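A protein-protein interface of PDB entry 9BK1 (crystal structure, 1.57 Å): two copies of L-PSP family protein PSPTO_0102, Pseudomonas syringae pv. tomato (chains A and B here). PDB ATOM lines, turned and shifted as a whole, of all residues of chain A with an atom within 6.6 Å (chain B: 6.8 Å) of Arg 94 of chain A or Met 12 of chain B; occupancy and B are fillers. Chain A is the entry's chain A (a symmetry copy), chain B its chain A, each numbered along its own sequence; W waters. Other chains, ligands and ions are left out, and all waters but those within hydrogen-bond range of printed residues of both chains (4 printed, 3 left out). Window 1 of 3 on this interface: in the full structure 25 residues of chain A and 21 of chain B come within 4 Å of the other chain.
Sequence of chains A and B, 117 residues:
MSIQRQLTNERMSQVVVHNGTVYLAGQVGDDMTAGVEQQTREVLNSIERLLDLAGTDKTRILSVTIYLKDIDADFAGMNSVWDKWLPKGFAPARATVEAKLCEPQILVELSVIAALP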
ATOM      1  N   LEU A  62      21.689   9.570  19.776  1.00  0.00           N
ATOM      2  CA  LEU A  62      20.833   9.984  18.674  1.00  0.00           C
ATOM      3  C   LEU A  62      19.850   8.895  18.277  1.00  0.00           C
ATOM      4  O   LEU A  62      18.660   9.177  18.085  1.00  0.00           O
ATOM      5  CB  LEU A  62      21.680  10.388  17.458  1.00  0.00           C
ATOM      6  CG  LEU A  62      22.762  11.445  17.698  1.00  0.00           C
ATOM      7  CD1 LEU A  62      23.583  11.645  16.439  1.00  0.00           C
ATOM      8  CD2 LEU A  62      22.141  12.766  18.165  1.00  0.00           C
ATOM      9  N   SER A  63      20.328   7.653  18.166  1.00  0.00           N
ATOM     10  CA  SER A  63      19.494   6.572  17.651  1.00  0.00           C
ATOM     11  C   SER A  63      20.027   5.251  18.186  1.00  0.00           C
ATOM     12  O   SER A  63      21.241   5.035  18.204  1.00  0.00           O
ATOM     13  CB  SER A  63      19.503   6.573  16.116  1.00  0.00           C
ATOM     14  OG  SER A  63      18.718   5.519  15.583  1.00  0.00           O
ATOM     15  N   VAL A  64      19.129   4.373  18.634  1.00  0.00           N
ATOM     16  CA  VAL A  64      19.520   3.062  19.140  1.00  0.00           C
ATOM     17  C   VAL A  64      18.627   2.023  18.495  1.00  0.00           C
ATOM     18  O   VAL A  64      17.400   2.188  18.451  1.00  0.00           O
ATOM     19  CB  VAL A  64      19.422   2.964  20.676  1.00  0.00           C
ATOM     20  CG1 VAL A  64      19.840   1.583  21.158  1.00  0.00           C
ATOM     21  CG2 VAL A  64      20.313   4.009  21.298  1.00  0.00           C
ATOM     22  N   THR A  65      19.237   0.967  17.985  1.00  0.00           N
ATOM     23  CA  THR A  65      18.497  -0.194  17.521  1.00  0.00           C
ATOM     24  C   THR A  65      18.742  -1.326  18.503  1.00  0.00           C
ATOM     25  O   THR A  65      19.891  -1.612  18.864  1.00  0.00           O
ATOM     26  CB  THR A  65      18.887  -0.584  16.096  1.00  0.00           C
ATOM     27  OG1 THR A  65      18.500   0.475  15.208  1.00  0.00           O
ATOM     28  CG2 THR A  65      18.170  -1.865  15.685  1.00  0.00           C
ATOM     29  N   ILE A  66      17.654  -1.928  18.968  1.00  0.00           N
ATOM     30  CA  ILE A  66      17.681  -2.947  20.006  1.00  0.00           C
ATOM     31  C   ILE A  66      17.257  -4.257  19.371  1.00  0.00           C
ATOM     32  O   ILE A  66      16.170  -4.334  18.789  1.00  0.00           O
ATOM     33  CB  ILE A  66      16.735  -2.596  21.160  1.00  0.00           C
ATOM     34  CG1 ILE A  66      17.163  -1.276  21.805  1.00  0.00           C
ATOM     35  CG2 ILE A  66      16.709  -3.716  22.192  1.00  0.00           C
ATOM     36  CD1 ILE A  66      16.179  -0.722  22.801  1.00  0.00           C
ATOM     37  N   PHE A  75      10.528  -8.211  25.550  1.00  0.00           N
ATOM     38  CA  PHE A  75      10.301  -6.795  25.271  1.00  0.00           C
ATOM     39  C   PHE A  75      10.015  -6.023  26.553  1.00  0.00           C
ATOM     40  O   PHE A  75      10.619  -4.977  26.814  1.00  0.00           O
ATOM     41  CB  PHE A  75       9.147  -6.664  24.277  1.00  0.00           C
ATOM     42  CG  PHE A  75       8.852  -5.251  23.822  1.00  0.00           C
ATOM     43  CD1 PHE A  75       9.815  -4.492  23.167  1.00  0.00           C
ATOM     44  CD2 PHE A  75       7.586  -4.710  23.991  1.00  0.00           C
ATOM     45  CE1 PHE A  75       9.527  -3.211  22.718  1.00  0.00           C
ATOM     46  CE2 PHE A  75       7.291  -3.431  23.543  1.00  0.00           C
ATOM     47  CZ  PHE A  75       8.271  -2.682  22.903  1.00  0.00           C
ATOM     48  N   MET A  78      13.123  -5.844  28.987  1.00  0.00           N
ATOM     49  CA  MET A  78      14.093  -4.898  28.456  1.00  0.00           C
ATOM     50  C   MET A  78      13.621  -3.462  28.668  1.00  0.00           C
ATOM     51  O   MET A  78      14.392  -2.603  29.121  1.00  0.00           O
ATOM     52  CB  MET A  78      14.333  -5.196  26.967  1.00  0.00           C
ATOM     53  CG  MET A  78      15.383  -4.304  26.291  1.00  0.00           C
ATOM     54  SD  MET A  78      14.754  -2.694  25.772  1.00  0.00           S
ATOM     55  CE  MET A  78      13.521  -3.203  24.575  1.00  0.00           C
ATOM     56  N   ASN A  79      12.354  -3.182  28.336  1.00  0.00           N
ATOM     57  CA  ASN A  79      11.821  -1.833  28.514  1.00  0.00           C
ATOM     58  C   ASN A  79      11.893  -1.392  29.964  1.00  0.00           C
ATOM     59  O   ASN A  79      12.120  -0.210  30.243  1.00  0.00           O
ATOM     60  CB  ASN A  79      10.374  -1.758  28.036  1.00  0.00           C
ATOM     61  CG  ASN A  79      10.256  -1.778  26.542  1.00  0.00           C
ATOM     62  OD1 ASN A  79      11.174  -1.372  25.835  1.00  0.00           O
ATOM     63  ND2 ASN A  79       9.125  -2.250  26.048  1.00  0.00           N
ATOM     64  N   TRP A  82      15.341  -0.070  30.202  1.00  0.00           N
ATOM     65  CA  TRP A  82      15.606   1.008  29.251  1.00  0.00           C
ATOM     66  C   TRP A  82      14.913   2.302  29.668  1.00  0.00           C
ATOM     67  O   TRP A  82      15.516   3.384  29.635  1.00  0.00           O
ATOM     68  CB  TRP A  82      15.156   0.593  27.844  1.00  0.00           C
ATOM     69  CG  TRP A  82      15.185   1.761  26.902  1.00  0.00           C
ATOM     70  CD1 TRP A  82      14.191   2.673  26.703  1.00  0.00           C
ATOM     71  CD2 TRP A  82      16.284   2.182  26.087  1.00  0.00           C
ATOM     72  NE1 TRP A  82      14.597   3.632  25.807  1.00  0.00           N
ATOM     73  CE2 TRP A  82      15.877   3.345  25.408  1.00  0.00           C
ATOM     74  CE3 TRP A  82      17.570   1.680  25.860  1.00  0.00           C
ATOM     75  CZ2 TRP A  82      16.705   4.018  24.510  1.00  0.00           C
ATOM     76  CZ3 TRP A  82      18.389   2.344  24.963  1.00  0.00           C
ATOM     77  CH2 TRP A  82      17.956   3.501  24.303  1.00  0.00           C
ATOM     78  N   ASP A  83      13.637   2.207  30.056  1.00  0.00           N
ATOM     79  CA  ASP A  83      12.819   3.380  30.328  1.00  0.00           C
ATOM     80  C   ASP A  83      13.347   4.198  31.500  1.00  0.00           C
ATOM     81  O   ASP A  83      12.973   5.369  31.633  1.00  0.00           O
ATOM     82  CB  ASP A  83      11.366   2.952  30.600  1.00  0.00           C
ATOM     83  CG  ASP A  83      10.648   2.426  29.355  1.00  0.00           C
ATOM     84  OD1 ASP A  83      11.177   2.571  28.233  1.00  0.00           O
ATOM     85  OD2 ASP A  83       9.538   1.857  29.494  1.00  0.00           O
ATOM     86  N   ALA A  91      15.725  11.217  25.458  1.00  0.00           N
ATOM     87  CA  ALA A  91      15.661   9.900  24.840  1.00  0.00           C
ATOM     88  C   ALA A  91      15.945   9.990  23.340  1.00  0.00           C
ATOM     89  O   ALA A  91      15.517  10.937  22.675  1.00  0.00           O
ATOM     90  CB  ALA A  91      14.291   9.260  25.069  1.00  0.00           C
ATOM     91  N   PRO A  92      16.662   9.022  22.793  1.00  0.00           N
ATOM     92  CA  PRO A  92      16.977   9.007  21.360  1.00  0.00           C
ATOM     93  C   PRO A  92      15.841   8.397  20.549  1.00  0.00           C
ATOM     94  O   PRO A  92      14.854   7.898  21.089  1.00  0.00           O
ATOM     95  CB  PRO A  92      18.209   8.113  21.313  1.00  0.00           C
ATOM     96  CG  PRO A  92      17.928   7.088  22.391  1.00  0.00           C
ATOM     97  CD  PRO A  92      17.276   7.895  23.510  1.00  0.00           C
ATOM     98  N   ALA A  93      16.009   8.425  19.226  1.00  0.00           N
ATOM     99  CA  ALA A  93      15.237   7.537  18.371  1.00  0.00           C
ATOM    100  C   ALA A  93      15.530   6.098  18.770  1.00  0.00           C
ATOM    101  O   ALA A  93      16.664   5.763  19.130  1.00  0.00           O
ATOM    102  CB  ALA A  93      15.602   7.762  16.897  1.00  0.00           C
ATOM    103  N   ARG A  94      14.505   5.242  18.705  1.00  0.00           N
ATOM    104  CA  ARG A  94      14.636   3.855  19.126  1.00  0.00           C
ATOM    105  C   ARG A  94      13.873   2.933  18.181  1.00  0.00           C
ATOM    106  O   ARG A  94      12.785   3.275  17.709  1.00  0.00           O
ATOM    107  CB  ARG A  94      14.126   3.668  20.570  1.00  0.00           C
ATOM    108  CG  ARG A  94      14.700   2.436  21.289  1.00  0.00           C
ATOM    109  CD  ARG A  94      14.053   2.218  22.645  1.00  0.00           C
ATOM    110  NE  ARG A  94      12.863   1.382  22.528  1.00  0.00           N
ATOM    111  CZ  ARG A  94      12.392   0.607  23.495  1.00  0.00           C
ATOM    112  NH1 ARG A  94      12.968   0.553  24.685  1.00  0.00           N
ATOM    113  NH2 ARG A  94      11.313  -0.131  23.258  1.00  0.00           N
ATOM    114  N   ALA A  95      14.452   1.763  17.902  1.00  0.00           N
ATOM    115  CA  ALA A  95      13.759   0.699  17.186  1.00  0.00           C
ATOM    116  C   ALA A  95      14.135  -0.621  17.832  1.00  0.00           C
ATOM    117  O   ALA A  95      15.298  -0.820  18.193  1.00  0.00           O
ATOM    118  CB  ALA A  95      14.127   0.675  15.695  1.00  0.00           C
ATOM    119  N   THR A  96      13.153  -1.510  17.985  1.00  0.00           N
ATOM    120  CA  THR A  96      13.325  -2.767  18.712  1.00  0.00           C
ATOM    121  C   THR A  96      12.739  -3.902  17.879  1.00  0.00           C
ATOM    122  O   THR A  96      11.556  -3.862  17.517  1.00  0.00           O
ATOM    123  CB  THR A  96      12.633  -2.692  20.076  1.00  0.00           C
ATOM    124  OG1 THR A  96      13.132  -1.561  20.801  1.00  0.00           O
ATOM    125  CG2 THR A  96      12.875  -3.947  20.884  1.00  0.00           C
ATOM    126  N   GLN B   6      12.201  15.849  19.172  1.00  0.00           N
ATOM    127  CA  GLN B   6      10.774  16.117  19.048  1.00  0.00           C
ATOM    128  C   GLN B   6       9.980  14.848  19.315  1.00  0.00           C
ATOM    129  O   GLN B   6      10.401  13.734  18.958  1.00  0.00           O
ATOM    130  CB  GLN B   6      10.398  16.654  17.660  1.00  0.00           C
ATOM    131  CG  GLN B   6      11.072  17.942  17.265  1.00  0.00           C
ATOM    132  CD  GLN B   6      10.438  18.534  16.024  1.00  0.00           C
ATOM    133  OE1 GLN B   6       9.215  18.612  15.926  1.00  0.00           O
ATOM    134  NE2 GLN B   6      11.259  18.934  15.063  1.00  0.00           N
ATOM    135  N   LEU B   7       8.806  15.049  19.925  1.00  0.00           N
ATOM    136  CA  LEU B   7       7.855  13.997  20.287  1.00  0.00           C
ATOM    137  C   LEU B   7       8.526  12.963  21.199  1.00  0.00           C
ATOM    138  O   LEU B   7       8.755  11.803  20.841  1.00  0.00           O
ATOM    139  CB  LEU B   7       7.249  13.354  19.032  1.00  0.00           C
ATOM    140  CG  LEU B   7       6.466  14.296  18.100  1.00  0.00           C
ATOM    141  CD1 LEU B   7       5.794  13.517  16.968  1.00  0.00           C
ATOM    142  CD2 LEU B   7       5.437  15.128  18.861  1.00  0.00           C
ATOM    143  N   THR B   8       8.833  13.433  22.403  1.00  0.00           N
ATOM    144  CA  THR B   8       9.706  12.740  23.341  1.00  0.00           C
ATOM    145  C   THR B   8       8.894  12.212  24.512  1.00  0.00           C
ATOM    146  O   THR B   8       8.039  12.924  25.051  1.00  0.00           O
ATOM    147  CB  THR B   8      10.804  13.681  23.854  1.00  0.00           C
ATOM    148  OG1 THR B   8      11.562  14.191  22.751  1.00  0.00           O
ATOM    149  CG2 THR B   8      11.736  12.966  24.818  1.00  0.00           C
ATOM    150  N   ASN B   9       9.149  10.962  24.887  1.00  0.00           N
ATOM    151  CA  ASN B   9       8.721  10.461  26.187  1.00  0.00           C
ATOM    152  C   ASN B   9       9.912   9.791  26.868  1.00  0.00           C
ATOM    153  O   ASN B   9      11.052   9.936  26.411  1.00  0.00           O
ATOM    154  CB  ASN B   9       7.519   9.516  26.047  1.00  0.00           C
ATOM    155  CG  ASN B   9       7.801   8.315  25.151  1.00  0.00           C
ATOM    156  OD1 ASN B   9       8.931   7.853  25.039  1.00  0.00           O
ATOM    157  ND2 ASN B   9       6.756   7.806  24.506  1.00  0.00           N
ATOM    158  N   GLU B  10       9.672   9.084  27.974  1.00  0.00           N
ATOM    159  CA  GLU B  10      10.769   8.488  28.724  1.00  0.00           C
ATOM    160  C   GLU B  10      11.525   7.450  27.912  1.00  0.00           C
ATOM    161  O   GLU B  10      12.701   7.189  28.190  1.00  0.00           O
ATOM    162  CB  GLU B  10      10.241   7.841  30.005  1.00  0.00           C
ATOM    163  CG  GLU B  10       9.894   8.825  31.120  1.00  0.00           C
ATOM    164  CD  GLU B  10       8.659   9.667  30.821  1.00  0.00           C
ATOM    165  OE1 GLU B  10       7.811   9.230  30.006  1.00  0.00           O
ATOM    166  OE2 GLU B  10       8.542  10.772  31.405  1.00  0.00           O
ATOM    167  N   ARG B  11      10.877   6.864  26.912  1.00  0.00           N
ATOM    168  CA  ARG B  11      11.457   5.750  26.177  1.00  0.00           C
ATOM    169  C   ARG B  11      12.162   6.196  24.906  1.00  0.00           C
ATOM    170  O   ARG B  11      13.216   5.645  24.563  1.00  0.00           O
ATOM    171  CB  ARG B  11      10.365   4.738  25.836  1.00  0.00           C
ATOM    172  CG  ARG B  11      10.839   3.537  25.044  1.00  0.00           C
ATOM    173  CD  ARG B  11       9.688   2.576  24.847  1.00  0.00           C
ATOM    174  NE  ARG B  11       9.257   2.005  26.118  1.00  0.00           N
ATOM    175  CZ  ARG B  11       8.220   1.187  26.245  1.00  0.00           C
ATOM    176  NH1 ARG B  11       7.480   0.850  25.202  1.00  0.00           N
ATOM    177  NH2 ARG B  11       7.927   0.689  27.443  1.00  0.00           N
ATOM    178  N   MET B  12      11.603   7.161  24.184  1.00  0.00           N
ATOM    179  CA  MET B  12      12.185   7.515  22.897  1.00  0.00           C
ATOM    180  C   MET B  12      11.704   8.888  22.469  1.00  0.00           C
ATOM    181  O   MET B  12      10.707   9.408  22.975  1.00  0.00           O
ATOM    182  CB  MET B  12      11.827   6.481  21.816  1.00  0.00           C
ATOM    183  CG  MET B  12      10.354   6.508  21.374  1.00  0.00           C
ATOM    184  SD  MET B  12       9.955   5.220  20.171  1.00  0.00           S
ATOM    185  CE  MET B  12       9.959   3.756  21.223  1.00  0.00           C
ATOM    186  N   SER B  13      12.429   9.469  21.523  1.00  0.00           N
ATOM    187  CA  SER B  13      11.956  10.596  20.734  1.00  0.00           C
ATOM    188  C   SER B  13      11.605  10.083  19.350  1.00  0.00           C
ATOM    189  O   SER B  13      12.352   9.281  18.780  1.00  0.00           O
ATOM    190  CB  SER B  13      13.018  11.690  20.610  1.00  0.00           C
ATOM    191  OG  SER B  13      13.319  12.265  21.866  1.00  0.00           O
ATOM    192  N   GLN B  14      10.480  10.550  18.801  1.00  0.00           N
ATOM    193  CA  GLN B  14      10.161  10.160  17.433  1.00  0.00           C
ATOM    194  C   GLN B  14      11.133  10.781  16.446  1.00  0.00           C
ATOM    195  O   GLN B  14      11.407  10.182  15.393  1.00  0.00           O
ATOM    196  CB  GLN B  14       8.735  10.561  17.058  1.00  0.00           C
ATOM    197  CG  GLN B  14       7.643   9.905  17.885  1.00  0.00           C
ATOM    198  CD  GLN B  14       7.736   8.398  17.854  1.00  0.00           C
ATOM    199  OE1 GLN B  14       7.739   7.797  16.787  1.00  0.00           O
ATOM    200  NE2 GLN B  14       7.838   7.785  19.018  1.00  0.00           N
ATOM    201  N   VAL B  15      11.644  11.979  16.759  1.00  0.00           N
ATOM    202  CA  VAL B  15      12.515  12.736  15.864  1.00  0.00           C
ATOM    203  C   VAL B  15      13.747  13.183  16.633  1.00  0.00           C
ATOM    204  O   VAL B  15      13.622  13.805  17.696  1.00  0.00           O
ATOM    205  CB  VAL B  15      11.801  13.970  15.284  1.00  0.00           C
ATOM    206  CG1 VAL B  15      12.779  14.819  14.482  1.00  0.00           C
ATOM    207  CG2 VAL B  15      10.595  13.559  14.441  1.00  0.00           C
ATOM    208  N   VAL B  16      14.935  12.923  16.082  1.00  0.00           N
ATOM    209  CA  VAL B  16      16.168  13.498  16.611  1.00  0.00           C
ATOM    210  C   VAL B  16      16.945  14.082  15.446  1.00  0.00           C
ATOM    211  O   VAL B  16      17.153  13.408  14.436  1.00  0.00           O
ATOM    212  CB  VAL B  16      17.023  12.465  17.375  1.00  0.00           C
ATOM    213  CG1 VAL B  16      18.341  13.100  17.856  1.00  0.00           C
ATOM    214  CG2 VAL B  16      16.241  11.890  18.561  1.00  0.00           C
ATOM    215  N   LEU B  24      14.855   8.999  12.760  1.00  0.00           N
ATOM    216  CA  LEU B  24      13.499   8.745  13.226  1.00  0.00           C
ATOM    217  C   LEU B  24      13.445   7.450  14.031  1.00  0.00           C
ATOM    218  O   LEU B  24      14.152   6.485  13.724  1.00  0.00           O
ATOM    219  CB  LEU B  24      12.507   8.671  12.060  1.00  0.00           C
ATOM    220  CG  LEU B  24      12.425   9.886  11.129  1.00  0.00           C
ATOM    221  CD1 LEU B  24      11.287   9.686  10.118  1.00  0.00           C
ATOM    222  CD2 LEU B  24      12.212  11.166  11.944  1.00  0.00           C
ATOM    223  N   ALA B  25      12.621   7.450  15.080  1.00  0.00           N
ATOM    224  CA  ALA B  25      12.271   6.212  15.771  1.00  0.00           C
ATOM    225  C   ALA B  25      11.612   5.242  14.794  1.00  0.00           C
ATOM    226  O   ALA B  25      11.065   5.634  13.762  1.00  0.00           O
ATOM    227  CB  ALA B  25      11.326   6.501  16.945  1.00  0.00           C
ATOM    228  N   GLY B  26      11.676   3.949  15.121  1.00  0.00           N
ATOM    229  CA  GLY B  26      11.038   2.961  14.268  1.00  0.00           C
ATOM    230  C   GLY B  26       9.545   3.222  14.167  1.00  0.00           C
ATOM    231  O   GLY B  26       8.887   3.520  15.161  1.00  0.00           O
ATOM    232  N   GLN B  27       9.014   3.115  12.946  1.00  0.00           N
ATOM    233  CA  GLN B  27       7.620   3.450  12.673  1.00  0.00           C
ATOM    234  C   GLN B  27       6.866   2.200  12.253  1.00  0.00           C
ATOM    235  O   GLN B  27       7.377   1.390  11.473  1.00  0.00           O
ATOM    236  CB  GLN B  27       7.502   4.515  11.575  1.00  0.00           C
ATOM    237  CG  GLN B  27       8.144   5.855  11.935  1.00  0.00           C
ATOM    238  CD  GLN B  27       7.552   6.457  13.189  1.00  0.00           C
ATOM    239  OE1 GLN B  27       6.335   6.666  13.280  1.00  0.00           O
ATOM    240  NE2 GLN B  27       8.398   6.735  14.168  1.00  0.00           N
ATOM    241  N   GLU B 109       8.004  -2.575   9.878  1.00  0.00           N
ATOM    242  CA  GLU B 109       8.512  -1.442  10.643  1.00  0.00           C
ATOM    243  C   GLU B 109       9.665  -0.820   9.876  1.00  0.00           C
ATOM    244  O   GLU B 109      10.501  -1.541   9.325  1.00  0.00           O
ATOM    245  CB  GLU B 109       8.982  -1.862  12.043  1.00  0.00           C
ATOM    246  CG  GLU B 109       9.542  -0.701  12.878  1.00  0.00           C
ATOM    247  CD  GLU B 109       9.646  -0.996  14.362  1.00  0.00           C
ATOM    248  OE1 GLU B 109       8.960  -1.916  14.870  1.00  0.00           O
ATOM    249  OE2 GLU B 109      10.423  -0.295  15.048  1.00  0.00           O
ATOM    250  N   SER B 111      12.899   2.035   9.875  1.00  0.00           N
ATOM    251  CA  SER B 111      13.858   2.924  10.537  1.00  0.00           C
ATOM    252  C   SER B 111      14.479   3.827   9.478  1.00  0.00           C
ATOM    253  O   SER B 111      15.122   3.331   8.551  1.00  0.00           O
ATOM    254  CB  SER B 111      14.951   2.121  11.242  1.00  0.00           C
ATOM    255  OG  SER B 111      14.490   1.557  12.455  1.00  0.00           O
HETATM  256  O   HOH W   1      10.330  -0.333  17.578  1.00  0.00           O
HETATM  257  O   HOH W   2      16.900   0.224  13.014  1.00  0.00           O
HETATM  258  O   HOH W   3      13.279  11.394  27.281  1.00  0.00           O
HETATM  259  O   HOH W   4       8.900  -3.547  17.130  1.00  0.00           O
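The backbone NH (N) of Ser 13 of chain B is in hydrogen-bond range of the backbone carbonyl oxygen (O) of Pro 92 of chain A, 2.9 Å away.
The side-chain hydroxyl (OG) of Ser 13 of chain B sits at hydrogen-bond distance from the backbone carbonyl oxygen (O) of Ala 91 of chain A (2.7 Å).
The guanidinium group of Arg 11 of chain B lies close to the side-chain amide nitrogen of Asn 79 of chain A (3.5 Å).
The backbone carbonyl oxygen (O) of Arg 94 of chain A sits at hydrogen-bond distance from the backbone NH (N) of Gly 26 of chain B (2.9 Å).
O of Arg 11 of chain B is in hydrogen-bond range of NE1 of Trp 82 of chain A, at 2.7 Å.
NH2 of Arg 11 of chain B lies within salt-bridge range of OD2 of Asp 83 of chain A, 2.9 Å away.
The side-chain amide oxygen (OD1) of Asn 9 of chain B sits at hydrogen-bond distance from the backbone NH (N) of Arg 11 of chain B, 2.9 Å away.
The side-chain hydroxyl (OG1) of Thr 8 of chain B is in hydrogen-bond range of the side-chain hydroxyl (OG) of Ser 13 of chain B (2.8 Å).
The guanidinium group (NH2) of Arg 94 of chain A is in hydrogen-bond range of the side-chain amide oxygen (OD1) of Asn 79 of chain A.
OG1 of Thr 96 of chain A lies within hydrogen-bond range of NH2 of Arg 94 of chain A (3.4 Å).
The backbone carbonyl oxygen (O) of Ala 95 of chain A lies within hydrogen-bond range of the backbone NH (N) of Ile 66 of chain A, 2.7 Å away.
N of Ala 25 of chain B lies within hydrogen-bond range of O of Gln 14 of chain B (3.0 Å).
Val 16 of chain B touches Leu 62 of chain A.
Ala 91 of chain A touches Asn 9 of chain B.
CB of Ala 91 of chain A touches CA of Met 12 of chain B (3.5 Å).
Pro 92 of chain A touches Met 12 of chain B (O to CA, 3.2 Å).
Ser 13 of chain B touches Ala 93 of chain A (O to CA, 3.4 Å).
Ala 93 of chain A touches Val 16 of chain B (N to CG2, 3.5 Å).
Ala 93 of chain A touches Leu 24 of chain B.
CB of Ala 93 of chain A touches N of Ala 25 of chain B, at 3.5 Å.
Arg 94 of chain A touches Met 12 of chain B.
Ala 95 of chain A touches Glu 109 of chain B.
Of the printed residues of chain B, Ala 93 of chain A touches Ser 13 (3.4 Å), Val 16 (3.5 Å), Leu 24 (3.6 Å) and Ala 25 (3.5 Å).
Printed residues of chain B within 4 Å of Ala 95 of chain A: Glu 109 and Ser 111.
Met 12 of chain B touches three residues of chain A.
Of the printed residues of chain A, Gly 26 of chain B touches Arg 94 (2.9 Å).
Printed residues of chain A within 4 Å of Glu 109 of chain B: Ala 95 (3.9 Å).
Of the 16 printed residues of chain A, 9 touch a printed residue of chain B.
Printed residues of chain A that touch a printed residue of chain B: Leu 62, Asn 79, Trp 82, Asp 83, Ala 91, Pro 92, Ala 93, Arg 94 and Ala 95.
Of the 17 printed residues of chain B, 11 touch a printed residue of chain A.
Hydrophobic or aromatic side chains of chain B within 4 Å of the printed part of chain A: Met 12, Val 16 and Ala 25.
Among the printed residues, 21 pairs touch across the chains.
No position is printed for both chains.
Water W1 lies within hydrogen-bond range of the side-chain carboxylate of Glu 109 of chain B (2.5 Å) and the backbone NH of Thr 96 of chain A (3.1 Å).
Water W4 bridges the backbone carbonyl oxygen (O) of Thr 96 of chain A (2.7 Å) and the side-chain carboxylate (OE1) of Glu 109 of chain B (2.8 Å).
Water W2 lies within hydrogen-bond range of OG1 of Thr 65 of chain A (2.7 Å) and OG of Ser 111 of chain B (2.8 Å).
Water W3 bridges O of Asn 9 of chain B and N of Ala 91 of chain A.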
